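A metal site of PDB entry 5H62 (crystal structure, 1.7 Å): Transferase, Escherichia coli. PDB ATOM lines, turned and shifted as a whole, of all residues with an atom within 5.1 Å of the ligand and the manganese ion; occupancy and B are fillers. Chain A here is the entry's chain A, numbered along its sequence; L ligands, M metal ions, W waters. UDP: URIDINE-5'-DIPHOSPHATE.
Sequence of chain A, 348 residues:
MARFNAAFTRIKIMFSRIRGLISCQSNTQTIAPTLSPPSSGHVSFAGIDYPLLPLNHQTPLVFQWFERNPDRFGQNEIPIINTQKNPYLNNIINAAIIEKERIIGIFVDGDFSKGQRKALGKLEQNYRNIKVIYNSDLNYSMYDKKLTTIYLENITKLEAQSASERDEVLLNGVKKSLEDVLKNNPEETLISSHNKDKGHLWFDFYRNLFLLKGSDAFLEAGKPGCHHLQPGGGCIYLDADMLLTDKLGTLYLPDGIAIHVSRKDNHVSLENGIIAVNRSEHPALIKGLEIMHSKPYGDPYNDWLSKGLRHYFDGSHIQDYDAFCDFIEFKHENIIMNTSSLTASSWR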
ATOM      1  N   GLN A  64       5.046 -16.365  14.147  1.00  0.00           N
ATOM      2  CA  GLN A  64       5.811 -17.222  13.271  1.00  0.00           C
ATOM      3  C   GLN A  64       6.909 -16.450  12.562  1.00  0.00           C
ATOM      4  O   GLN A  64       6.615 -15.321  12.111  1.00  0.00           O
ATOM      5  CB  GLN A  64       4.860 -17.824  12.246  1.00  0.00           C
ATOM      6  CG  GLN A  64       5.523 -18.686  11.182  1.00  0.00           C
ATOM      7  CD  GLN A  64       4.520 -19.194  10.176  1.00  0.00           C
ATOM      8  OE1 GLN A  64       3.569 -18.538   9.812  1.00  0.00           O
ATOM      9  NE2 GLN A  64       4.756 -20.466   9.687  1.00  0.00           N
ATOM     10  N   TRP A  65       8.133 -16.945  12.544  1.00  0.00           N
ATOM     11  CA  TRP A  65       9.123 -16.345  11.649  1.00  0.00           C
ATOM     12  C   TRP A  65       9.917 -17.467  10.940  1.00  0.00           C
ATOM     13  O   TRP A  65      10.758 -18.103  11.539  1.00  0.00           O
ATOM     14  CB  TRP A  65      10.055 -15.322  12.346  1.00  0.00           C
ATOM     15  CG  TRP A  65      10.793 -14.577  11.309  1.00  0.00           C
ATOM     16  CD1 TRP A  65      12.117 -14.769  10.928  1.00  0.00           C
ATOM     17  CD2 TRP A  65      10.252 -13.645  10.394  1.00  0.00           C
ATOM     18  NE1 TRP A  65      12.392 -13.949   9.855  1.00  0.00           N
ATOM     19  CE2 TRP A  65      11.256 -13.282   9.525  1.00  0.00           C
ATOM     20  CE3 TRP A  65       8.973 -13.095  10.193  1.00  0.00           C
ATOM     21  CZ2 TRP A  65      11.081 -12.400   8.488  1.00  0.00           C
ATOM     22  CZ3 TRP A  65       8.798 -12.213   9.156  1.00  0.00           C
ATOM     23  CH2 TRP A  65       9.880 -11.854   8.335  1.00  0.00           C
ATOM     24  N   PHE A  66       9.619 -17.620   9.654  1.00  0.00           N
ATOM     25  CA  PHE A  66      10.296 -18.579   8.807  1.00  0.00           C
ATOM     26  C   PHE A  66      11.241 -17.766   7.980  1.00  0.00           C
ATOM     27  O   PHE A  66      10.812 -16.926   7.174  1.00  0.00           O
ATOM     28  CB  PHE A  66       9.281 -19.365   7.952  1.00  0.00           C
ATOM     29  CG  PHE A  66       8.645 -20.535   8.625  1.00  0.00           C
ATOM     30  CD1 PHE A  66       8.489 -20.589   9.972  1.00  0.00           C
ATOM     31  CD2 PHE A  66       8.279 -21.607   7.883  1.00  0.00           C
ATOM     32  CE1 PHE A  66       7.955 -21.702  10.615  1.00  0.00           C
ATOM     33  CE2 PHE A  66       7.702 -22.731   8.462  1.00  0.00           C
ATOM     34  CZ  PHE A  66       7.524 -22.824   9.841  1.00  0.00           C
ATOM     35  N   GLU A  67      12.526 -18.023   8.109  1.00  0.00           N
ATOM     36  CA  GLU A  67      13.535 -17.167   7.506  1.00  0.00           C
ATOM     37  C   GLU A  67      14.291 -17.906   6.415  1.00  0.00           C
ATOM     38  O   GLU A  67      15.035 -18.841   6.698  1.00  0.00           O
ATOM     39  CB  GLU A  67      14.502 -16.695   8.586  1.00  0.00           C
ATOM     40  CG  GLU A  67      15.640 -15.869   8.058  1.00  0.00           C
ATOM     41  CD  GLU A  67      15.143 -14.696   7.307  1.00  0.00           C
ATOM     42  OE1 GLU A  67      15.567 -14.556   6.111  1.00  0.00           O
ATOM     43  OE2 GLU A  67      14.358 -13.872   7.851  1.00  0.00           O
ATOM     44  N   ARG A  72      21.515 -13.225   6.251  1.00  0.00           N
ATOM     45  CA  ARG A  72      21.418 -11.772   6.238  1.00  0.00           C
ATOM     46  C   ARG A  72      21.468 -11.127   7.627  1.00  0.00           C
ATOM     47  O   ARG A  72      21.559  -9.916   7.750  1.00  0.00           O
ATOM     48  CB  ARG A  72      20.167 -11.310   5.495  1.00  0.00           C
ATOM     49  CG  ARG A  72      18.816 -11.548   6.202  1.00  0.00           C
ATOM     50  CD  ARG A  72      17.634 -11.349   5.244  1.00  0.00           C
ATOM     51  NE  ARG A  72      16.354 -11.686   5.854  1.00  0.00           N
ATOM     52  CZ  ARG A  72      15.241 -10.943   5.817  1.00  0.00           C
ATOM     53  NH1 ARG A  72      15.214  -9.771   5.154  1.00  0.00           N
ATOM     54  NH2 ARG A  72      14.116 -11.399   6.410  1.00  0.00           N
ATOM     55  N   ASN A  86       9.543  -3.049   9.246  1.00  0.00           N
ATOM     56  CA  ASN A  86       9.047  -4.320   9.757  1.00  0.00           C
ATOM     57  C   ASN A  86       9.703  -4.682  11.068  1.00  0.00           C
ATOM     58  O   ASN A  86      10.550  -5.600  11.180  1.00  0.00           O
ATOM     59  CB  ASN A  86       9.294  -5.420   8.723  1.00  0.00           C
ATOM     60  CG  ASN A  86       8.628  -5.120   7.401  1.00  0.00           C
ATOM     61  OD1 ASN A  86       9.315  -4.724   6.462  1.00  0.00           O
ATOM     62  ND2 ASN A  86       7.325  -5.254   7.317  1.00  0.00           N
ATOM     63  N   TYR A  88       9.386  -6.515  13.517  1.00  0.00           N
ATOM     64  CA  TYR A  88       8.648  -7.625  14.010  1.00  0.00           C
ATOM     65  C   TYR A  88       9.113  -8.275  15.305  1.00  0.00           C
ATOM     66  O   TYR A  88       8.297  -8.668  16.157  1.00  0.00           O
ATOM     67  CB  TYR A  88       8.515  -8.679  12.906  1.00  0.00           C
ATOM     68  CG  TYR A  88       7.646  -8.245  11.730  1.00  0.00           C
ATOM     69  CD1 TYR A  88       6.939  -7.021  11.716  1.00  0.00           C
ATOM     70  CD2 TYR A  88       7.493  -9.072  10.641  1.00  0.00           C
ATOM     71  CE1 TYR A  88       6.182  -6.651  10.639  1.00  0.00           C
ATOM     72  CE2 TYR A  88       6.688  -8.697   9.579  1.00  0.00           C
ATOM     73  CZ  TYR A  88       6.067  -7.487   9.588  1.00  0.00           C
ATOM     74  OH  TYR A  88       5.324  -7.088   8.520  1.00  0.00           O
ATOM     75  N   PHE A 203       5.627 -20.656   4.835  1.00  0.00           N
ATOM     76  CA  PHE A 203       5.040 -20.297   6.118  1.00  0.00           C
ATOM     77  C   PHE A 203       3.577 -20.489   6.158  1.00  0.00           C
ATOM     78  O   PHE A 203       3.056 -20.887   7.203  1.00  0.00           O
ATOM     79  CB  PHE A 203       5.470 -18.893   6.663  1.00  0.00           C
ATOM     80  CG  PHE A 203       5.539 -17.798   5.657  1.00  0.00           C
ATOM     81  CD1 PHE A 203       6.739 -17.482   5.071  1.00  0.00           C
ATOM     82  CD2 PHE A 203       4.456 -16.977   5.417  1.00  0.00           C
ATOM     83  CE1 PHE A 203       6.873 -16.355   4.198  1.00  0.00           C
ATOM     84  CE2 PHE A 203       4.583 -15.887   4.597  1.00  0.00           C
ATOM     85  CZ  PHE A 203       5.794 -15.602   3.939  1.00  0.00           C
ATOM     86  N   ARG A 207       1.975 -22.923   9.050  1.00  0.00           N
ATOM     87  CA  ARG A 207       1.092 -22.240  10.013  1.00  0.00           C
ATOM     88  C   ARG A 207      -0.131 -23.056  10.260  1.00  0.00           C
ATOM     89  O   ARG A 207      -0.513 -23.239  11.382  1.00  0.00           O
ATOM     90  CB  ARG A 207       0.694 -20.874   9.430  1.00  0.00           C
ATOM     91  CG  ARG A 207      -0.083 -20.001  10.344  1.00  0.00           C
ATOM     92  CD  ARG A 207      -0.382 -18.676   9.681  1.00  0.00           C
ATOM     93  NE  ARG A 207       0.838 -17.967   9.381  1.00  0.00           N
ATOM     94  CZ  ARG A 207       0.913 -16.829   8.691  1.00  0.00           C
ATOM     95  NH1 ARG A 207      -0.148 -16.202   8.258  1.00  0.00           N
ATOM     96  NH2 ARG A 207       2.105 -16.324   8.376  1.00  0.00           N
ATOM     97  N   TYR A 237      -2.907 -17.556  16.988  1.00  0.00           N
ATOM     98  CA  TYR A 237      -1.853 -17.246  16.044  1.00  0.00           C
ATOM     99  C   TYR A 237      -2.049 -15.826  15.564  1.00  0.00           C
ATOM    100  O   TYR A 237      -3.188 -15.451  15.102  1.00  0.00           O
ATOM    101  CB  TYR A 237      -1.830 -18.210  14.818  1.00  0.00           C
ATOM    102  CG  TYR A 237      -0.936 -17.640  13.787  1.00  0.00           C
ATOM    103  CD1 TYR A 237       0.428 -17.736  13.947  1.00  0.00           C
ATOM    104  CD2 TYR A 237      -1.430 -16.757  12.810  1.00  0.00           C
ATOM    105  CE1 TYR A 237       1.309 -17.065  13.117  1.00  0.00           C
ATOM    106  CE2 TYR A 237      -0.589 -16.092  11.994  1.00  0.00           C
ATOM    107  CZ  TYR A 237       0.802 -16.212  12.156  1.00  0.00           C
ATOM    108  OH  TYR A 237       1.671 -15.507  11.349  1.00  0.00           O
ATOM    109  N   ASP A 239      -0.021 -12.749  13.016  1.00  0.00           N
ATOM    110  CA  ASP A 239       1.066 -12.120  12.281  1.00  0.00           C
ATOM    111  C   ASP A 239       1.772 -11.097  13.193  1.00  0.00           C
ATOM    112  O   ASP A 239       1.094 -10.496  14.062  1.00  0.00           O
ATOM    113  CB  ASP A 239       0.542 -11.396  11.065  1.00  0.00           C
ATOM    114  CG  ASP A 239       0.285 -12.316   9.879  1.00  0.00           C
ATOM    115  OD1 ASP A 239       0.535 -13.542   9.968  1.00  0.00           O
ATOM    116  OD2 ASP A 239      -0.145 -11.772   8.794  1.00  0.00           O
ATOM    117  N   ALA A 240       3.081 -10.937  13.024  1.00  0.00           N
ATOM    118  CA  ALA A 240       3.881 -10.051  13.869  1.00  0.00           C
ATOM    119  C   ALA A 240       3.567  -8.590  13.740  1.00  0.00           C
ATOM    120  O   ALA A 240       3.886  -7.825  14.651  1.00  0.00           O
ATOM    121  CB  ALA A 240       5.344 -10.339  13.693  1.00  0.00           C
ATOM    122  N   ASP A 241       2.845  -8.207  12.723  1.00  0.00           N
ATOM    123  CA  ASP A 241       2.323  -6.848  12.562  1.00  0.00           C
ATOM    124  C   ASP A 241       0.946  -6.587  13.146  1.00  0.00           C
ATOM    125  O   ASP A 241       0.377  -5.527  12.938  1.00  0.00           O
ATOM    126  CB  ASP A 241       2.354  -6.438  11.094  1.00  0.00           C
ATOM    127  CG  ASP A 241       1.311  -7.096  10.300  1.00  0.00           C
ATOM    128  OD1 ASP A 241       0.627  -7.997  10.775  1.00  0.00           O
ATOM    129  OD2 ASP A 241       1.161  -6.677   9.160  1.00  0.00           O
ATOM    130  N   ASN A 338      -2.786  -5.905  10.852  1.00  0.00           N
ATOM    131  CA  ASN A 338      -2.083  -5.836   9.603  1.00  0.00           C
ATOM    132  C   ASN A 338      -1.375  -4.531   9.325  1.00  0.00           C
ATOM    133  O   ASN A 338      -1.530  -3.931   8.271  1.00  0.00           O
ATOM    134  CB  ASN A 338      -3.030  -6.178   8.462  1.00  0.00           C
ATOM    135  CG  ASN A 338      -2.335  -6.513   7.171  1.00  0.00           C
ATOM    136  OD1 ASN A 338      -1.127  -6.614   7.081  1.00  0.00           O
ATOM    137  ND2 ASN A 338      -3.096  -6.560   6.145  1.00  0.00           N
ATOM    138  N   THR A 339      -0.544  -4.122  10.294  1.00  0.00           N
ATOM    139  CA  THR A 339       0.142  -2.860  10.105  1.00  0.00           C
ATOM    140  C   THR A 339       1.143  -2.800   9.014  1.00  0.00           C
ATOM    141  O   THR A 339       1.495  -1.716   8.595  1.00  0.00           O
ATOM    142  CB  THR A 339       0.726  -2.288  11.433  1.00  0.00           C
ATOM    143  OG1 THR A 339       1.692  -3.210  11.968  1.00  0.00           O
ATOM    144  CG2 THR A 339      -0.292  -2.100  12.430  1.00  0.00           C
ATOM    145  N   SER A 340       1.594  -3.945   8.438  1.00  0.00           N
ATOM    146  CA  SER A 340       2.465  -3.917   7.351  1.00  0.00           C
ATOM    147  C   SER A 340       1.772  -3.259   6.165  1.00  0.00           C
ATOM    148  O   SER A 340       2.437  -2.744   5.322  1.00  0.00           O
ATOM    149  CB  SER A 340       2.923  -5.325   6.919  1.00  0.00           C
ATOM    150  OG  SER A 340       1.837  -6.028   6.350  1.00  0.00           O
ATOM    151  N   SER A 341       0.448  -3.349   6.105  1.00  0.00           N
ATOM    152  CA  SER A 341      -0.260  -2.773   4.994  1.00  0.00           C
ATOM    153  C   SER A 341      -0.135  -1.266   4.949  1.00  0.00           C
ATOM    154  O   SER A 341      -0.346  -0.642   3.939  1.00  0.00           O
ATOM    155  CB  SER A 341      -1.705  -3.191   4.970  1.00  0.00           C
ATOM    156  OG  SER A 341      -2.419  -2.833   6.128  1.00  0.00           O
ATOM    157  N   ALA A 344       5.223  -1.578   4.761  1.00  0.00           N
ATOM    158  CA  ALA A 344       5.429  -2.473   3.611  1.00  0.00           C
ATOM    159  C   ALA A 344       5.398  -3.935   4.030  1.00  0.00           C
ATOM    160  O   ALA A 344       5.774  -4.276   5.114  1.00  0.00           O
ATOM    161  CB  ALA A 344       6.736  -2.171   2.912  1.00  0.00           C
ATOM    162  N   SER A 345       4.993  -4.788   3.119  1.00  0.00           N
ATOM    163  CA  SER A 345       5.000  -6.235   3.394  1.00  0.00           C
ATOM    164  C   SER A 345       6.421  -6.686   3.569  1.00  0.00           C
ATOM    165  O   SER A 345       7.369  -6.177   2.925  1.00  0.00           O
ATOM    166  CB  SER A 345       4.440  -6.953   2.202  1.00  0.00           C
ATOM    167  OG  SER A 345       4.646  -8.355   2.330  1.00  0.00           O
ATOM    168  N   SER A 346       6.634  -7.634   4.445  1.00  0.00           N
ATOM    169  CA  SER A 346       8.010  -8.131   4.625  1.00  0.00           C
ATOM    170  C   SER A 346       8.449  -9.130   3.578  1.00  0.00           C
ATOM    171  O   SER A 346       9.572  -9.681   3.701  1.00  0.00           O
ATOM    172  CB  SER A 346       8.112  -8.780   5.982  1.00  0.00           C
ATOM    173  OG  SER A 346       7.178  -9.884   6.026  1.00  0.00           O
ATOM    174  N   TRP A 347       7.557  -9.454   2.644  1.00  0.00           N
ATOM    175  CA  TRP A 347       7.884 -10.433   1.587  1.00  0.00           C
ATOM    176  C   TRP A 347       7.284 -10.159   0.224  1.00  0.00           C
ATOM    177  O   TRP A 347       7.835 -10.634  -0.756  1.00  0.00           O
ATOM    178  CB  TRP A 347       7.496 -11.866   2.036  1.00  0.00           C
ATOM    179  CG  TRP A 347       6.038 -12.100   2.180  1.00  0.00           C
ATOM    180  CD1 TRP A 347       5.274 -11.882   3.331  1.00  0.00           C
ATOM    181  CD2 TRP A 347       5.107 -12.523   1.179  1.00  0.00           C
ATOM    182  NE1 TRP A 347       3.995 -12.186   3.091  1.00  0.00           N
ATOM    183  CE2 TRP A 347       3.855 -12.563   1.776  1.00  0.00           C
ATOM    184  CE3 TRP A 347       5.225 -12.899  -0.177  1.00  0.00           C
ATOM    185  CZ2 TRP A 347       2.697 -12.959   1.088  1.00  0.00           C
ATOM    186  CZ3 TRP A 347       4.099 -13.288  -0.858  1.00  0.00           C
ATOM    187  CH2 TRP A 347       2.835 -13.313  -0.223  1.00  0.00           C
ATOM    188  N   ARG A 348       6.166  -9.448   0.095  1.00  0.00           N
ATOM    189  CA  ARG A 348       5.530  -9.295  -1.247  1.00  0.00           C
ATOM    190  C   ARG A 348       6.343  -8.534  -2.298  1.00  0.00           C
ATOM    191  O   ARG A 348       7.072  -7.640  -1.912  1.00  0.00           O
ATOM    192  CB  ARG A 348       4.208  -8.604  -1.146  1.00  0.00           C
ATOM    193  CG  ARG A 348       3.157  -9.519  -0.556  1.00  0.00           C
ATOM    194  CD  ARG A 348       1.899  -8.749  -0.238  1.00  0.00           C
ATOM    195  NE  ARG A 348       1.125  -9.551   0.692  1.00  0.00           N
ATOM    196  CZ  ARG A 348       0.318 -10.549   0.362  1.00  0.00           C
ATOM    197  NH1 ARG A 348       0.166 -10.912  -0.915  1.00  0.00           N
ATOM    198  NH2 ARG A 348      -0.313 -11.236   1.298  1.00  0.00           N
HETATM  199  N1  UDP L   1       6.567 -14.336   7.309  1.00  0.00           N
HETATM  200  C2  UDP L   1       7.639 -15.228   7.534  1.00  0.00           C
HETATM  201  N3  UDP L   1       8.774 -15.079   6.906  1.00  0.00           N
HETATM  202  C4  UDP L   1       8.929 -14.098   6.010  1.00  0.00           C
HETATM  203  C5  UDP L   1       7.942 -13.155   5.791  1.00  0.00           C
HETATM  204  C6  UDP L   1       6.758 -13.281   6.443  1.00  0.00           C
HETATM  205  O2  UDP L   1       7.478 -16.156   8.368  1.00  0.00           O
HETATM  206  O4  UDP L   1      10.081 -13.960   5.471  1.00  0.00           O
HETATM  207  C1' UDP L   1       5.312 -14.601   8.064  1.00  0.00           C
HETATM  208  C2' UDP L   1       5.389 -13.951   9.443  1.00  0.00           C
HETATM  209  O2' UDP L   1       4.709 -14.853  10.299  1.00  0.00           O
HETATM  210  C3' UDP L   1       4.745 -12.607   9.251  1.00  0.00           C
HETATM  211  C4' UDP L   1       3.604 -13.000   8.269  1.00  0.00           C
HETATM  212  O4' UDP L   1       4.274 -13.896   7.363  1.00  0.00           O
HETATM  213  O3' UDP L   1       4.147 -12.172  10.493  1.00  0.00           O
HETATM  214  C5' UDP L   1       2.968 -11.856   7.494  1.00  0.00           C
HETATM  215  O5' UDP L   1       4.017 -10.974   7.059  1.00  0.00           O
HETATM  216  PA  UDP L   1       3.526  -9.510   6.599  1.00  0.00           P
HETATM  217  O1A UDP L   1       2.524  -8.991   7.606  1.00  0.00           O
HETATM  218  O2A UDP L   1       4.766  -8.806   6.441  1.00  0.00           O
HETATM  219  O3A UDP L   1       2.858  -9.842   5.175  1.00  0.00           O
HETATM  220  PB  UDP L   1       1.509  -9.414   4.440  1.00  0.00           P
HETATM  221  O1B UDP L   1       2.022  -8.623   3.301  1.00  0.00           O
HETATM  222  O2B UDP L   1       0.625  -8.675   5.381  1.00  0.00           O
HETATM  223  O3B UDP L   1       0.863 -10.714   4.056  1.00  0.00           O
HETATM  224 MN    MN M   1       0.719  -7.800   7.294  1.00  0.00          MN
HETATM  225  O   HOH W   1       3.477  -9.420  10.107  1.00  0.00           O
HETATM  226  O   HOH W   2       1.382 -13.287   4.564  1.00  0.00           O
HETATM  227  O   HOH W   3      12.070 -15.535   4.395  1.00  0.00           O
HETATM  228  O   HOH W   4       3.571 -14.179  13.082  1.00  0.00           O
HETATM  229  O   HOH W   5      -1.310  -7.238   3.916  1.00  0.00           O
HETATM  230  O   HOH W   6       1.778  -6.017   3.874  1.00  0.00           O
HETATM  231  O   HOH W   7      11.123 -11.515   4.573  1.00  0.00           O
HETATM  232  O   HOH W   8      -0.369  -9.092   8.547  1.00  0.00           O
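Merely in contact with the ligand: Trp 65 (3.4 Å), Phe 203 (3.4 Å) and Asp 239 (3.4 Å). Hydrophobic or aromatic side chains that line the ligand: Trp 65, Phe 66, Tyr 88, Phe 203, Ala 240 and Trp 347. Within 4 Å of the ligand: Gln 64, Trp 65, Phe 66, Tyr 88, Phe 203, Arg 207, Tyr 237, Asp 239, Ala 240, Asp 241, Asn 338, Ser 340, Ser 345, Ser 346, Trp 347 and Arg 348. Along chain A the residues within 4 Å of the ligand span positions 64 to 348. The nearest printed residue that does not touch the ligand is Asn 86 (4.5 Å).
Water W8 lies within hydrogen-bond range of OD1 of Asp 241 and OD2 of Asp 239. Water W2 lies within hydrogen-bond range of an oxygen (O3B) of the ligand (2.7 Å) and the indole nitrogen (NE1) of Trp 347 (3.2 Å). Water W1 lies within hydrogen-bond range of an oxygen (O3') of the ligand (2.9 Å), the backbone NH of Asp 241 (3.0 Å), the backbone NH of Ala 240 (3.3 Å) and the side-chain hydroxyl of Tyr 88 (3.4 Å). Water W3 bridges O4 of the ligand (2.8 Å) and O of Phe 66 (3.4 Å). Water W7 lies within hydrogen-bond range of the backbone carbonyl oxygen of Ser 346 (2.6 Å) and an oxygen (O4) of the ligand (2.8 Å). Water W4 lies within hydrogen-bond range of the backbone NH of Gln 64 (2.8 Å), the side-chain hydroxyl of Tyr 237 (2.9 Å), an oxygen (O2') of the ligand (3.1 Å) and the backbone NH of Ala 240 (3.3 Å).
Water W8 binds the manganese ion. The manganese ion is bound by O2B of the ligand (2.1 Å). The manganese ion is bound by O1A of the ligand (2.2 Å). OD1 of Asn 338 is bound to the manganese ion (2.2 Å). The manganese ion is bound by OD2 of Asp 241 (2.2 Å). OG of Ser 340 is bound to the manganese ion, 2.3 Å away. The manganese ion has six donor atoms within binding distance.
Three residues have an atom within 4 Å of the manganese ion: Asp 241, Asn 338 and Ser 340.
The backbone carbonyl oxygen (O) of Gln 64 sits at hydrogen-bond distance from an oxygen (O2') of the ligand (2.7 Å). The backbone NH of Ser 346 lies within hydrogen-bond range of an oxygen (O2A) of the ligand, 3.0 Å away. OG of Ser 346 is in hydrogen-bond range of O2A of the ligand. The side-chain hydroxyl (OH) of Tyr 88 sits at hydrogen-bond distance from an oxygen (O2A) of the ligand (2.8 Å). The backbone NH of Phe 66 sits at hydrogen-bond distance from an oxygen (O2) of the ligand. A nitrogen (N3) of the ligand is in hydrogen-bond range of the backbone carbonyl oxygen (O) of Phe 66. The side-chain hydroxyl (OG) of Ser 345 sits at hydrogen-bond distance from an oxygen (O1B) of the ligand, at 2.8 Å. The guanidinium group (NE) of Arg 348 lies within salt-bridge range of an oxygen (O1B) of the ligand (2.9 Å). O3' of the ligand sits at hydrogen-bond distance from N of Ala 240, at 3.0 Å. O2' of the ligand lies within hydrogen-bond range of OH of Tyr 237 (3.3 Å). The indole nitrogen (NE1) of Trp 347 sits at hydrogen-bond distance from an oxygen (O3A) of the ligand, 3.3 Å away. The guanidinium group of Arg 207 sits at hydrogen-bond distance from an oxygen (O4') of the ligand (3.4 Å).
The backbone carbonyl oxygen (O) of Asn 338 lies within hydrogen-bond range of the side-chain hydroxyl (OG) of Ser 341, 2.6 Å away. The side-chain amide oxygen (OE1) of Gln 64 lies within hydrogen-bond range of the guanidinium group (NE) of Arg 207, 2.8 Å away. O of Phe 203 lies within hydrogen-bond range of NE2 of Gln 64 (3.0 Å). OH of Tyr 88 lies within hydrogen-bond range of ND2 of Asn 86. OG of Ser 345 sits at hydrogen-bond distance from N of Trp 347 (3.1 Å). The side-chain hydroxyl of Tyr 237 sits at hydrogen-bond distance from the side-chain carboxylate of Asp 239 (2.7 Å). The side-chain hydroxyl (OH) of Tyr 237 sits close to the guanidinium group (NH2) of Arg 207, at 3.1 Å. NE1 of Trp 65 sits at hydrogen-bond distance from OE2 of Glu 67, at 2.8 Å.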
